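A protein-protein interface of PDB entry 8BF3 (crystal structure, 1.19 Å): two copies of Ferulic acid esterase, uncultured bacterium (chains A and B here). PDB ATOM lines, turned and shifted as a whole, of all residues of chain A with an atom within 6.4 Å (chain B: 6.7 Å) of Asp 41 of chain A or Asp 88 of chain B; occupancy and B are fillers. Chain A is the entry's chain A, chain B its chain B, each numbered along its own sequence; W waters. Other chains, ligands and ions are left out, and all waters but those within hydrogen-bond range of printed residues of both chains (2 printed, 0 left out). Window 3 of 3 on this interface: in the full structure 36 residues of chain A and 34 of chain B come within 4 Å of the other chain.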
ATOM      1  N   TYR A  38     -10.782  -4.227 -15.883  1.00  0.00           N
ATOM      2  CA  TYR A  38     -11.535  -2.977 -15.894  1.00  0.00           C
ATOM      3  C   TYR A  38     -11.633  -2.413 -17.305  1.00  0.00           C
ATOM      4  O   TYR A  38     -10.617  -2.230 -17.986  1.00  0.00           O
ATOM      5  CB  TYR A  38     -10.894  -1.928 -14.989  1.00  0.00           C
ATOM      6  CG  TYR A  38     -11.602  -0.597 -15.081  1.00  0.00           C
ATOM      7  CD1 TYR A  38     -12.761  -0.354 -14.358  1.00  0.00           C
ATOM      8  CD2 TYR A  38     -11.136   0.402 -15.923  1.00  0.00           C
ATOM      9  CE1 TYR A  38     -13.424   0.865 -14.453  1.00  0.00           C
ATOM     10  CE2 TYR A  38     -11.790   1.616 -16.028  1.00  0.00           C
ATOM     11  CZ  TYR A  38     -12.933   1.841 -15.290  1.00  0.00           C
ATOM     12  OH  TYR A  38     -13.586   3.051 -15.392  1.00  0.00           O
ATOM     13  N   SER A  39     -12.858  -2.099 -17.726  1.00  0.00           N
ATOM     14  CA  SER A  39     -13.055  -1.261 -18.899  1.00  0.00           C
ATOM     15  C   SER A  39     -14.511  -0.887 -19.065  1.00  0.00           C
ATOM     16  O   SER A  39     -15.372  -1.761 -19.188  1.00  0.00           O
ATOM     17  CB  SER A  39     -12.624  -1.952 -20.187  1.00  0.00           C
ATOM     18  OG  SER A  39     -13.040  -1.150 -21.283  1.00  0.00           O
ATOM     19  N   LYS A  40     -14.791   0.406 -19.105  1.00  0.00           N
ATOM     20  CA  LYS A  40     -16.136   0.859 -19.420  1.00  0.00           C
ATOM     21  C   LYS A  40     -16.443   0.778 -20.905  1.00  0.00           C
ATOM     22  O   LYS A  40     -17.612   0.812 -21.280  1.00  0.00           O
ATOM     23  CB  LYS A  40     -16.348   2.286 -18.927  1.00  0.00           C
ATOM     24  CG  LYS A  40     -16.458   2.379 -17.416  1.00  0.00           C
ATOM     25  CD  LYS A  40     -16.835   3.788 -16.989  1.00  0.00           C
ATOM     26  CE  LYS A  40     -17.030   3.900 -15.488  1.00  0.00           C
ATOM     27  NZ  LYS A  40     -17.458   5.277 -15.109  1.00  0.00           N
ATOM     28  N   ASP A  41     -15.430   0.667 -21.752  1.00  0.00           N
ATOM     29  CA  ASP A  41     -15.661   0.659 -23.188  1.00  0.00           C
ATOM     30  C   ASP A  41     -16.003  -0.732 -23.711  1.00  0.00           C
ATOM     31  O   ASP A  41     -16.841  -0.857 -24.613  1.00  0.00           O
ATOM     32  CB  ASP A  41     -14.428   1.201 -23.911  1.00  0.00           C
ATOM     33  CG  ASP A  41     -14.193   2.668 -23.630  1.00  0.00           C
ATOM     34  OD1 ASP A  41     -14.959   3.498 -24.149  1.00  0.00           O
ATOM     35  OD2 ASP A  41     -13.250   2.992 -22.875  1.00  0.00           O
ATOM     36  N   ALA A  42     -15.376  -1.772 -23.152  1.00  0.00           N
ATOM     37  CA  ALA A  42     -15.422  -3.096 -23.747  1.00  0.00           C
ATOM     38  C   ALA A  42     -16.801  -3.721 -23.653  1.00  0.00           C
ATOM     39  O   ALA A  42     -17.532  -3.529 -22.684  1.00  0.00           O
ATOM     40  CB  ALA A  42     -14.387  -4.005 -23.078  1.00  0.00           C
ATOM     41  N   SER A  43     -17.155  -4.481 -24.691  1.00  0.00           N
ATOM     42  CA  SER A  43     -18.417  -5.215 -24.709  1.00  0.00           C
ATOM     43  C   SER A  43     -18.295  -6.582 -24.051  1.00  0.00           C
ATOM     44  O   SER A  43     -19.114  -6.948 -23.200  1.00  0.00           O
ATOM     45  CB  SER A  43     -18.919  -5.415 -26.143  1.00  0.00           C
ATOM     46  OG  SER A  43     -20.053  -6.283 -26.152  1.00  0.00           O
ATOM     47  N   LYS A  63     -19.827  -8.154 -16.492  1.00  0.00           N
ATOM     48  CA  LYS A  63     -19.580  -6.729 -16.335  1.00  0.00           C
ATOM     49  C   LYS A  63     -20.549  -6.158 -15.309  1.00  0.00           C
ATOM     50  O   LYS A  63     -21.746  -6.456 -15.347  1.00  0.00           O
ATOM     51  CB  LYS A  63     -19.775  -6.010 -17.673  1.00  0.00           C
ATOM     52  CG  LYS A  63     -19.232  -4.576 -17.717  1.00  0.00           C
ATOM     53  CD  LYS A  63     -19.455  -3.940 -19.083  1.00  0.00           C
ATOM     54  CE  LYS A  63     -18.685  -2.635 -19.235  1.00  0.00           C
ATOM     55  NZ  LYS A  63     -18.771  -2.101 -20.631  1.00  0.00           N
ATOM     56  N   PHE A  69     -15.189  -6.038 -15.075  1.00  0.00           N
ATOM     57  CA  PHE A  69     -15.520  -7.398 -15.457  1.00  0.00           C
ATOM     58  C   PHE A  69     -14.885  -8.347 -14.451  1.00  0.00           C
ATOM     59  O   PHE A  69     -13.732  -8.151 -14.042  1.00  0.00           O
ATOM     60  CB  PHE A  69     -14.919  -7.713 -16.827  1.00  0.00           C
ATOM     61  CG  PHE A  69     -15.567  -6.991 -17.992  1.00  0.00           C
ATOM     62  CD1 PHE A  69     -15.217  -5.685 -18.311  1.00  0.00           C
ATOM     63  CD2 PHE A  69     -16.476  -7.647 -18.804  1.00  0.00           C
ATOM     64  CE1 PHE A  69     -15.782  -5.053 -19.406  1.00  0.00           C
ATOM     65  CE2 PHE A  69     -17.032  -7.014 -19.895  1.00  0.00           C
ATOM     66  CZ  PHE A  69     -16.688  -5.711 -20.192  1.00  0.00           C
ATOM     67  N   VAL A  87     -10.431  -9.579 -25.197  1.00  0.00           N
ATOM     68  CA  VAL A  87     -11.225  -8.364 -25.065  1.00  0.00           C
ATOM     69  C   VAL A  87     -11.731  -8.016 -26.450  1.00  0.00           C
ATOM     70  O   VAL A  87     -10.945  -7.661 -27.332  1.00  0.00           O
ATOM     71  CB  VAL A  87     -10.386  -7.213 -24.497  1.00  0.00           C
ATOM     72  CG1 VAL A  87     -11.203  -5.925 -24.467  1.00  0.00           C
ATOM     73  CG2 VAL A  87      -9.832  -7.559 -23.131  1.00  0.00           C
ATOM     74  N   ASP A  88     -13.036  -8.138 -26.660  1.00  0.00           N
ATOM     75  CA  ASP A  88     -13.643  -7.823 -27.948  1.00  0.00           C
ATOM     76  C   ASP A  88     -12.819  -8.418 -29.086  1.00  0.00           C
ATOM     77  O   ASP A  88     -12.528  -7.765 -30.090  1.00  0.00           O
ATOM     78  CB  ASP A  88     -13.846  -6.321 -28.104  1.00  0.00           C
ATOM     79  CG  ASP A  88     -14.817  -5.768 -27.092  1.00  0.00           C
ATOM     80  OD1 ASP A  88     -15.672  -6.538 -26.620  1.00  0.00           O
ATOM     81  OD2 ASP A  88     -14.743  -4.567 -26.761  1.00  0.00           O
ATOM     82  N   ASP B  41     -14.580  -7.572 -33.964  1.00  0.00           N
ATOM     83  CA  ASP B  41     -15.463  -7.217 -32.863  1.00  0.00           C
ATOM     84  C   ASP B  41     -14.982  -6.036 -32.042  1.00  0.00           C
ATOM     85  O   ASP B  41     -15.717  -5.578 -31.164  1.00  0.00           O
ATOM     86  CB  ASP B  41     -15.641  -8.420 -31.933  1.00  0.00           C
ATOM     87  CG  ASP B  41     -16.325  -9.567 -32.618  1.00  0.00           C
ATOM     88  OD1 ASP B  41     -17.242  -9.294 -33.416  1.00  0.00           O
ATOM     89  OD2 ASP B  41     -15.951 -10.728 -32.367  1.00  0.00           O
ATOM     90  N   ALA B  42     -13.774  -5.547 -32.270  1.00  0.00           N
ATOM     91  CA  ALA B  42     -13.284  -4.425 -31.491  1.00  0.00           C
ATOM     92  C   ALA B  42     -13.750  -3.116 -32.106  1.00  0.00           C
ATOM     93  O   ALA B  42     -13.949  -3.008 -33.319  1.00  0.00           O
ATOM     94  CB  ALA B  42     -11.759  -4.448 -31.413  1.00  0.00           C
ATOM     95  N   SER B  43     -13.922  -2.113 -31.251  1.00  0.00           N
ATOM     96  CA  SER B  43     -14.365  -0.797 -31.685  1.00  0.00           C
ATOM     97  C   SER B  43     -13.210   0.164 -31.912  1.00  0.00           C
ATOM     98  O   SER B  43     -13.175   0.866 -32.930  1.00  0.00           O
ATOM     99  CB  SER B  43     -15.299  -0.202 -30.633  1.00  0.00           C
ATOM    100  OG  SER B  43     -15.780   1.048 -31.071  1.00  0.00           O
ATOM    101  N   LYS B  44     -12.261   0.206 -30.977  1.00  0.00           N
ATOM    102  CA  LYS B  44     -11.203   1.204 -30.986  1.00  0.00           C
ATOM    103  C   LYS B  44      -9.914   0.553 -30.516  1.00  0.00           C
ATOM    104  O   LYS B  44      -9.904  -0.165 -29.512  1.00  0.00           O
ATOM    105  CB  LYS B  44     -11.566   2.362 -30.055  1.00  0.00           C
ATOM    106  CG  LYS B  44     -10.500   3.416 -29.876  1.00  0.00           C
ATOM    107  CD  LYS B  44     -11.110   4.715 -29.363  1.00  0.00           C
ATOM    108  CE  LYS B  44     -10.086   5.567 -28.642  1.00  0.00           C
ATOM    109  NZ  LYS B  44     -10.066   6.966 -29.139  1.00  0.00           N
ATOM    110  N   VAL B  45      -8.830   0.796 -31.244  1.00  0.00           N
ATOM    111  CA  VAL B  45      -7.501   0.361 -30.839  1.00  0.00           C
ATOM    112  C   VAL B  45      -6.583   1.565 -30.938  1.00  0.00           C
ATOM    113  O   VAL B  45      -6.528   2.227 -31.981  1.00  0.00           O
ATOM    114  CB  VAL B  45      -6.978  -0.787 -31.717  1.00  0.00           C
ATOM    115  CG1 VAL B  45      -5.598  -1.228 -31.255  1.00  0.00           C
ATOM    116  CG2 VAL B  45      -7.954  -1.968 -31.708  1.00  0.00           C
ATOM    117  N   THR B  46      -5.868   1.850 -29.857  1.00  0.00           N
ATOM    118  CA  THR B  46      -4.848   2.888 -29.873  1.00  0.00           C
ATOM    119  C   THR B  46      -3.492   2.260 -29.594  1.00  0.00           C
ATOM    120  O   THR B  46      -3.393   1.098 -29.192  1.00  0.00           O
ATOM    121  CB  THR B  46      -5.139   3.986 -28.838  1.00  0.00           C
ATOM    122  OG1 THR B  46      -5.027   3.432 -27.526  1.00  0.00           O
ATOM    123  CG2 THR B  46      -6.534   4.579 -29.032  1.00  0.00           C
ATOM    124  N   PHE B  69      -7.129  -3.356 -37.905  1.00  0.00           N
ATOM    125  CA  PHE B  69      -6.732  -2.032 -37.450  1.00  0.00           C
ATOM    126  C   PHE B  69      -5.264  -1.831 -37.788  1.00  0.00           C
ATOM    127  O   PHE B  69      -4.451  -2.741 -37.604  1.00  0.00           O
ATOM    128  CB  PHE B  69      -6.863  -1.937 -35.928  1.00  0.00           C
ATOM    129  CG  PHE B  69      -8.270  -1.956 -35.416  1.00  0.00           C
ATOM    130  CD1 PHE B  69      -8.965  -3.146 -35.262  1.00  0.00           C
ATOM    131  CD2 PHE B  69      -8.886  -0.773 -35.041  1.00  0.00           C
ATOM    132  CE1 PHE B  69     -10.269  -3.144 -34.765  1.00  0.00           C
ATOM    133  CE2 PHE B  69     -10.173  -0.765 -34.532  1.00  0.00           C
ATOM    134  CZ  PHE B  69     -10.862  -1.949 -34.391  1.00  0.00           C
ATOM    135  N   THR B  86      -4.000  -0.369 -26.718  1.00  0.00           N
ATOM    136  CA  THR B  86      -5.158  -0.360 -25.834  1.00  0.00           C
ATOM    137  C   THR B  86      -6.347  -0.705 -26.715  1.00  0.00           C
ATOM    138  O   THR B  86      -6.613  -0.006 -27.698  1.00  0.00           O
ATOM    139  CB  THR B  86      -5.354   1.001 -25.165  1.00  0.00           C
ATOM    140  OG1 THR B  86      -4.149   1.382 -24.490  1.00  0.00           O
ATOM    141  CG2 THR B  86      -6.494   0.949 -24.149  1.00  0.00           C
ATOM    142  N   VAL B  87      -7.027  -1.800 -26.386  1.00  0.00           N
ATOM    143  CA  VAL B  87      -8.165  -2.297 -27.149  1.00  0.00           C
ATOM    144  C   VAL B  87      -9.404  -2.067 -26.304  1.00  0.00           C
ATOM    145  O   VAL B  87      -9.542  -2.654 -25.229  1.00  0.00           O
ATOM    146  CB  VAL B  87      -8.019  -3.797 -27.459  1.00  0.00           C
ATOM    147  CG1 VAL B  87      -9.269  -4.317 -28.196  1.00  0.00           C
ATOM    148  CG2 VAL B  87      -6.748  -4.069 -28.237  1.00  0.00           C
ATOM    149  N   ASP B  88     -10.307  -1.219 -26.778  1.00  0.00           N
ATOM    150  CA  ASP B  88     -11.560  -0.961 -26.073  1.00  0.00           C
ATOM    151  C   ASP B  88     -11.315  -0.776 -24.577  1.00  0.00           C
ATOM    152  O   ASP B  88     -12.004  -1.347 -23.725  1.00  0.00           O
ATOM    153  CB  ASP B  88     -12.572  -2.066 -26.357  1.00  0.00           C
ATOM    154  CG  ASP B  88     -12.968  -2.115 -27.815  1.00  0.00           C
ATOM    155  OD1 ASP B  88     -12.705  -1.110 -28.502  1.00  0.00           O
ATOM    156  OD2 ASP B  88     -13.549  -3.133 -28.276  1.00  0.00           O
ATOM    157  N   GLY B  89     -10.300   0.033 -24.268  1.00  0.00           N
ATOM    158  CA  GLY B  89      -9.988   0.431 -22.919  1.00  0.00           C
ATOM    159  C   GLY B  89      -9.088  -0.492 -22.128  1.00  0.00           C
ATOM    160  O   GLY B  89      -8.818  -0.199 -20.959  1.00  0.00           O
ATOM    161  N   VAL B  90      -8.620  -1.597 -22.708  1.00  0.00           N
ATOM    162  CA  VAL B  90      -7.801  -2.578 -22.004  1.00  0.00           C
ATOM    163  C   VAL B  90      -6.418  -2.639 -22.652  1.00  0.00           C
ATOM    164  O   VAL B  90      -6.299  -2.789 -23.873  1.00  0.00           O
ATOM    165  CB  VAL B  90      -8.461  -3.966 -22.016  1.00  0.00           C
ATOM    166  CG1 VAL B  90      -7.577  -4.968 -21.263  1.00  0.00           C
ATOM    167  CG2 VAL B  90      -9.852  -3.919 -21.400  1.00  0.00           C
HETATM  168  O   HOH W   1      -8.121  -1.301 -18.199  1.00  0.00           O
HETATM  169  O   HOH W   2     -15.569  -0.862 -27.037  1.00  0.00           O
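Hydrophobic or aromatic side chains of chain A that line the printed part of chain B: Ala 42 and Val 87.
Of the 12 printed residues of chain B, 6 touch a printed residue of chain A.
Printed residues of chain B that touch a printed residue of chain A: Asp 41, Ala 42, Val 87, Asp 88, Gly 89 and Val 90.
Hydrophobic or aromatic side chains of chain B that line the printed part of chain A: Ala 42, Val 87 and Val 90.
Along chain B the printed residues that touch a printed residue of chain A span positions 41 to 90.
Among the printed residues, 11 pairs touch across the chains.
Asp 41 of chain A touches Asp 88 of chain B, and with the chains exchanged Asp 88 of chain A touches Asp 41 of chain B.
Ala 42 of chain A touches Asp 88 of chain B, and with the chains exchanged Asp 88 of chain A touches Ala 42 of chain B.
Val 87 of chain B touches its own counterpart, Val 87 of chain A.
Asp 88 of chain A touches its own counterpart, Asp 88 of chain B.
Of the 11 pairs that touch across the chains among the printed residues, 6 have their exchanged pair printed and touching as well.
Water W1 bridges the backbone carbonyl oxygen (O) of Tyr 38 of chain A (2.7 Å) and the backbone carbonyl oxygen (O) of Gly 89 of chain B (3.1 Å).
Water W2 lies within hydrogen-bond range of the backbone carbonyl oxygen of Asp 41 of chain A and the side-chain carboxylate of Asp 88 of chain B.
Among the printed residues, merely in contact across the chains: Asp 41 of chain A with Asp 88 of chain B (3.5 Å), Asp 88 of chain A with Asp 41 of chain B (3.6 Å), Ser 39 of chain A with Val 90 of chain B (3.6 Å), Val 87 of chain A with Val 87 of chain B (3.7 Å), Ser 39 of chain A with Gly 89 of chain B (3.8 Å), Tyr 38 of chain A with Val 90 of chain B (3.9 Å) and Val 87 of chain A with Val 90 of chain B (3.9 Å).
Of the printed residues of chain B, Tyr 38 of chain A touches Val 90 (3.9 Å).
Of the printed residues of chain B, Asp 41 of chain A touches Asp 88 (3.5 Å).
Of the printed residues of chain B, Asp 88 of chain A touches Asp 41 (3.6 Å), Ala 42 (3.4 Å) and Asp 88 (2.4 Å).
Printed residues of chain A within 4 Å of Ala 42 of chain B: Asp 88.
Printed residues of chain A within 4 Å of Val 87 of chain B: Val 87.
The nearest printed residue of chain B that does not touch Asp 41 of chain A is Gly 89 of chain B (4.1 Å).
The backbone carbonyl oxygen (O) of Asp 88 of chain B sits at hydrogen-bond distance from the side-chain hydroxyl (OG) of Ser 39 of chain A, at 2.7 Å.
The backbone NH (N) of Ala 42 of chain A lies within hydrogen-bond range of the backbone carbonyl oxygen (O) of Asp 88 of chain B.
O of Asp 88 of chain A is in hydrogen-bond range of N of Ala 42 of chain B (3.4 Å).
OD2 of Asp 88 of chain B sits close to OD2 of Asp 88 of chain A, at 2.4 Å.
The side-chain hydroxyl of Ser 39 of chain A lies within hydrogen-bond range of the backbone NH of Asp 41 of chain A (3.0 Å).
OG of Ser 39 of chain A lies within hydrogen-bond range of N of Ala 42 of chain A, 3.1 Å away.
The side-chain amino group (NZ) of Lys 63 of chain A is in hydrogen-bond range of the backbone carbonyl oxygen (O) of Ala 42 of chain A, 2.8 Å away.
The backbone NH of Ser 43 of chain A is in hydrogen-bond range of the side-chain carboxylate of Asp 88 of chain A (3.2 Å).
OD2 of Asp 88 of chain B lies within hydrogen-bond range of N of Ser 43 of chain B.
The backbone NH (N) of Lys 44 of chain B sits at hydrogen-bond distance from the side-chain carboxylate (OD1) of Asp 88 of chain B (2.8 Å).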
